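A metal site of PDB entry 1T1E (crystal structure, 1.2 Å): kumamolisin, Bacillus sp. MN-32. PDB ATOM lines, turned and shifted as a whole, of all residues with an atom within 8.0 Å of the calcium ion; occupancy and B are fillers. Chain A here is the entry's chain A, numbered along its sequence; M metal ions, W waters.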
ATOM      1  N   VAL A 395      13.497 -25.677  21.418  1.00  0.00           N
ATOM      2  CA  VAL A 395      13.779 -26.889  22.195  1.00  0.00           C
ATOM      3  C   VAL A 395      15.294 -27.025  22.468  1.00  0.00           C
ATOM      4  O   VAL A 395      16.133 -26.771  21.588  1.00  0.00           O
ATOM      5  CB  VAL A 395      13.337 -28.142  21.426  1.00  0.00           C
ATOM      6  CG1 VAL A 395      13.636 -29.396  22.239  1.00  0.00           C
ATOM      7  CG2 VAL A 395      11.833 -28.062  21.103  1.00  0.00           C
ATOM      8  N   HIS A 503       4.330 -18.958  26.826  1.00  0.00           N
ATOM      9  CA  HIS A 503       5.095 -18.624  25.638  1.00  0.00           C
ATOM     10  C   HIS A 503       5.274 -19.965  24.966  1.00  0.00           C
ATOM     11  O   HIS A 503       5.960 -20.858  25.481  1.00  0.00           O
ATOM     12  CB  HIS A 503       6.451 -18.020  25.985  1.00  0.00           C
ATOM     13  CG  HIS A 503       7.250 -17.644  24.771  1.00  0.00           C
ATOM     14  ND1 HIS A 503       6.765 -16.758  23.827  1.00  0.00           N
ATOM     15  CD2 HIS A 503       8.452 -18.059  24.326  1.00  0.00           C
ATOM     16  CE1 HIS A 503       7.644 -16.649  22.841  1.00  0.00           C
ATOM     17  NE2 HIS A 503       8.678 -17.428  23.119  1.00  0.00           N
ATOM     18  N   ASP A 504       4.629 -20.134  23.823  1.00  0.00           N
ATOM     19  CA  ASP A 504       4.675 -21.378  23.085  1.00  0.00           C
ATOM     20  C   ASP A 504       6.010 -21.625  22.385  1.00  0.00           C
ATOM     21  O   ASP A 504       6.483 -20.761  21.662  1.00  0.00           O
ATOM     22  CB  ASP A 504       3.535 -21.336  22.063  1.00  0.00           C
ATOM     23  CG  ASP A 504       3.238 -22.676  21.452  1.00  0.00           C
ATOM     24  OD1 ASP A 504       3.931 -23.654  21.769  1.00  0.00           O
ATOM     25  OD2 ASP A 504       2.301 -22.783  20.629  1.00  0.00           O
ATOM     26  N   ILE A 505       6.632 -22.791  22.627  1.00  0.00           N
ATOM     27  CA  ILE A 505       7.853 -23.129  21.898  1.00  0.00           C
ATOM     28  C   ILE A 505       7.356 -23.976  20.718  1.00  0.00           C
ATOM     29  O   ILE A 505       6.631 -24.938  20.888  1.00  0.00           O
ATOM     30  CB  ILE A 505       8.856 -23.956  22.755  1.00  0.00           C
ATOM     31  CG1 ILE A 505       9.570 -23.048  23.781  1.00  0.00           C
ATOM     32  CG2 ILE A 505       9.923 -24.589  21.874  1.00  0.00           C
ATOM     33  CD1 ILE A 505       8.849 -22.890  25.094  1.00  0.00           C
ATOM     34  N   THR A 506       7.747 -23.602  19.502  1.00  0.00           N
ATOM     35  CA  THR A 506       7.267 -24.317  18.323  1.00  0.00           C
ATOM     36  C   THR A 506       8.343 -24.945  17.452  1.00  0.00           C
ATOM     37  O   THR A 506       8.031 -25.722  16.536  1.00  0.00           O
ATOM     38  CB  THR A 506       6.430 -23.369  17.440  1.00  0.00           C
ATOM     39  OG1 THR A 506       7.256 -22.274  17.030  1.00  0.00           O
ATOM     40  CG2 THR A 506       5.212 -22.813  18.226  1.00  0.00           C
ATOM     41  N   GLU A 507       9.601 -24.604  17.703  1.00  0.00           N
ATOM     42  CA  GLU A 507      10.688 -25.112  16.882  1.00  0.00           C
ATOM     43  C   GLU A 507      11.696 -25.973  17.646  1.00  0.00           C
ATOM     44  O   GLU A 507      12.100 -25.637  18.777  1.00  0.00           O
ATOM     45  CB  GLU A 507      11.399 -23.937  16.226  1.00  0.00           C
ATOM     46  CG  GLU A 507      10.497 -23.175  15.261  1.00  0.00           C
ATOM     47  CD  GLU A 507      11.236 -22.086  14.518  1.00  0.00           C
ATOM     48  OE1 GLU A 507      11.590 -21.067  15.150  1.00  0.00           O
ATOM     49  OE2 GLU A 507      11.474 -22.248  13.303  1.00  0.00           O
ATOM     50  N   GLN A 520       8.998 -33.929  18.391  1.00  0.00           N
ATOM     51  CA  GLN A 520       9.150 -32.595  17.845  1.00  0.00           C
ATOM     52  C   GLN A 520       8.190 -31.551  18.415  1.00  0.00           C
ATOM     53  O   GLN A 520       7.046 -31.877  18.752  1.00  0.00           O
ATOM     54  CB  GLN A 520       8.995 -32.663  16.330  1.00  0.00           C
ATOM     55  CG  GLN A 520       9.213 -31.360  15.591  1.00  0.00           C
ATOM     56  CD  GLN A 520       9.268 -31.575  14.104  1.00  0.00           C
ATOM     57  OE1 GLN A 520       8.320 -32.089  13.503  1.00  0.00           O
ATOM     58  NE2 GLN A 520      10.385 -31.199  13.485  1.00  0.00           N
ATOM     59  N   ALA A 521       8.645 -30.308  18.521  1.00  0.00           N
ATOM     60  CA  ALA A 521       7.824 -29.224  19.058  1.00  0.00           C
ATOM     61  C   ALA A 521       6.841 -28.753  17.977  1.00  0.00           C
ATOM     62  O   ALA A 521       6.993 -29.086  16.796  1.00  0.00           O
ATOM     63  CB  ALA A 521       8.691 -28.054  19.506  1.00  0.00           C
ATOM     64  N   GLY A 522       5.836 -27.988  18.397  1.00  0.00           N
ATOM     65  CA  GLY A 522       4.848 -27.492  17.453  1.00  0.00           C
ATOM     66  C   GLY A 522       3.893 -26.564  18.171  1.00  0.00           C
ATOM     67  O   GLY A 522       4.043 -26.327  19.359  1.00  0.00           O
ATOM     68  N   PRO A 523       2.903 -26.003  17.469  1.00  0.00           N
ATOM     69  CA  PRO A 523       1.936 -25.086  18.095  1.00  0.00           C
ATOM     70  C   PRO A 523       1.226 -25.829  19.231  1.00  0.00           C
ATOM     71  O   PRO A 523       0.845 -26.982  19.051  1.00  0.00           O
ATOM     72  CB  PRO A 523       0.963 -24.774  16.947  1.00  0.00           C
ATOM     73  CG  PRO A 523       1.806 -24.955  15.712  1.00  0.00           C
ATOM     74  CD  PRO A 523       2.616 -26.178  16.033  1.00  0.00           C
ATOM     75  N   GLY A 524       1.057 -25.198  20.380  1.00  0.00           N
ATOM     76  CA  GLY A 524       0.367 -25.844  21.491  1.00  0.00           C
ATOM     77  C   GLY A 524       1.261 -26.802  22.238  1.00  0.00           C
ATOM     78  O   GLY A 524       2.481 -26.696  22.196  1.00  0.00           O
ATOM     79  N   TRP A 525       0.670 -27.778  22.905  1.00  0.00           N
ATOM     80  CA  TRP A 525       1.452 -28.733  23.682  1.00  0.00           C
ATOM     81  C   TRP A 525       2.270 -29.672  22.799  1.00  0.00           C
ATOM     82  O   TRP A 525       1.779 -30.160  21.781  1.00  0.00           O
ATOM     83  CB  TRP A 525       0.496 -29.573  24.539  1.00  0.00           C
ATOM     84  CG  TRP A 525       1.181 -30.429  25.587  1.00  0.00           C
ATOM     85  CD1 TRP A 525       1.332 -30.120  26.904  1.00  0.00           C
ATOM     86  CD2 TRP A 525       1.850 -31.678  25.376  1.00  0.00           C
ATOM     87  NE1 TRP A 525       2.061 -31.101  27.542  1.00  0.00           N
ATOM     88  CE2 TRP A 525       2.401 -32.075  26.632  1.00  0.00           C
ATOM     89  CE3 TRP A 525       2.045 -32.501  24.269  1.00  0.00           C
ATOM     90  CZ2 TRP A 525       3.132 -33.253  26.793  1.00  0.00           C
ATOM     91  CZ3 TRP A 525       2.783 -33.677  24.423  1.00  0.00           C
ATOM     92  CH2 TRP A 525       3.318 -34.041  25.686  1.00  0.00           C
ATOM     93  N   ASP A 526       3.515 -29.935  23.193  1.00  0.00           N
ATOM     94  CA  ASP A 526       4.334 -30.915  22.464  1.00  0.00           C
ATOM     95  C   ASP A 526       5.163 -31.709  23.474  1.00  0.00           C
ATOM     96  O   ASP A 526       5.307 -31.292  24.638  1.00  0.00           O
ATOM     97  CB  ASP A 526       5.221 -30.250  21.389  1.00  0.00           C
ATOM     98  CG  ASP A 526       6.050 -29.129  21.931  1.00  0.00           C
ATOM     99  OD1 ASP A 526       6.968 -29.369  22.760  1.00  0.00           O
ATOM    100  OD2 ASP A 526       5.818 -27.983  21.531  1.00  0.00           O
ATOM    101  N   PRO A 527       5.690 -32.883  23.061  1.00  0.00           N
ATOM    102  CA  PRO A 527       6.478 -33.726  23.954  1.00  0.00           C
ATOM    103  C   PRO A 527       7.936 -33.318  24.139  1.00  0.00           C
ATOM    104  O   PRO A 527       8.768 -34.163  24.436  1.00  0.00           O
ATOM    105  CB  PRO A 527       6.337 -35.136  23.367  1.00  0.00           C
ATOM    106  CG  PRO A 527       5.391 -34.965  22.129  1.00  0.00           C
ATOM    107  CD  PRO A 527       5.515 -33.527  21.750  1.00  0.00           C
ATOM    108  N   CYS A 528       8.211 -32.038  23.946  1.00  0.00           N
ATOM    109  CA  CYS A 528       9.547 -31.495  24.193  1.00  0.00           C
ATOM    110  C   CYS A 528       9.450 -30.417  25.274  1.00  0.00           C
ATOM    111  O   CYS A 528      10.300 -30.350  26.186  1.00  0.00           O
ATOM    112  CB  CYS A 528      10.117 -30.841  22.942  1.00  0.00           C
ATOM    113  SG  CYS A 528      10.273 -31.890  21.500  1.00  0.00           S
ATOM    114  N   THR A 529       8.418 -29.581  25.180  1.00  0.00           N
ATOM    115  CA  THR A 529       8.251 -28.418  26.034  1.00  0.00           C
ATOM    116  C   THR A 529       6.881 -28.248  26.673  1.00  0.00           C
ATOM    117  O   THR A 529       6.656 -27.250  27.353  1.00  0.00           O
ATOM    118  CB  THR A 529       8.593 -27.131  25.243  1.00  0.00           C
ATOM    119  OG1 THR A 529       7.704 -26.998  24.113  1.00  0.00           O
ATOM    120  CG2 THR A 529      10.017 -27.208  24.720  1.00  0.00           C
ATOM    121  N   GLY A 530       5.989 -29.205  26.442  1.00  0.00           N
ATOM    122  CA  GLY A 530       4.657 -29.105  27.025  1.00  0.00           C
ATOM    123  C   GLY A 530       3.949 -27.829  26.606  1.00  0.00           C
ATOM    124  O   GLY A 530       3.939 -27.473  25.420  1.00  0.00           O
ATOM    125  N   LEU A 531       3.367 -27.126  27.577  1.00  0.00           N
ATOM    126  CA  LEU A 531       2.646 -25.891  27.295  1.00  0.00           C
ATOM    127  C   LEU A 531       3.545 -24.706  26.977  1.00  0.00           C
ATOM    128  O   LEU A 531       3.069 -23.635  26.606  1.00  0.00           O
ATOM    129  CB  LEU A 531       1.754 -25.541  28.499  1.00  0.00           C
ATOM    130  CG  LEU A 531       0.723 -26.614  28.861  1.00  0.00           C
ATOM    131  CD1 LEU A 531       0.073 -26.313  30.203  1.00  0.00           C
ATOM    132  CD2 LEU A 531      -0.368 -26.709  27.759  1.00  0.00           C
ATOM    133  N   GLY A 532       4.855 -24.893  27.119  1.00  0.00           N
ATOM    134  CA  GLY A 532       5.786 -23.809  26.863  1.00  0.00           C
ATOM    135  C   GLY A 532       6.321 -23.193  28.161  1.00  0.00           C
ATOM    136  O   GLY A 532       6.220 -23.805  29.238  1.00  0.00           O
ATOM    137  N   SER A 533       6.915 -22.012  28.069  1.00  0.00           N
ATOM    138  CA  SER A 533       7.423 -21.353  29.261  1.00  0.00           C
ATOM    139  C   SER A 533       6.314 -20.467  29.862  1.00  0.00           C
ATOM    140  O   SER A 533       5.653 -19.700  29.156  1.00  0.00           O
ATOM    141  CB  SER A 533       8.699 -20.548  28.958  1.00  0.00           C
ATOM    142  OG  SER A 533       8.532 -19.526  27.976  1.00  0.00           O
HETATM  143 CA    CA M   1       4.584 -25.923  21.614  1.00  0.00          CA
HETATM  144  O   HOH W   1       5.387 -25.598  23.899  1.00  0.00           O
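The side-chain carboxylate (OD1) of Asp 526 is in hydrogen-bond range of the side-chain hydroxyl (OG1) of Thr 529, at 2.8 Å.
N of Cys 528 sits close to OD1 of Asp 526, 3.2 Å away.
The calcium ion is bound by the backbone carbonyl oxygen (O) of Gly 524 (2.3 Å), the backbone carbonyl oxygen (O) of Gly 522 (2.4 Å), the side-chain carboxylate (OD1) of Asp 504 (2.4 Å), the backbone carbonyl oxygen (O) of Ile 505 (2.4 Å), the side-chain carboxylate (OD2) of Asp 526 (2.4 Å) and water W1 (2.4 Å).
The calcium ion has six donor atoms within binding distance.
Water W1 lies within hydrogen-bond range of the side-chain hydroxyl (OG1) of Thr 529, the backbone carbonyl oxygen (O) of Gly 530, the backbone NH (N) of Ile 505 and the backbone NH (N) of Gly 532.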
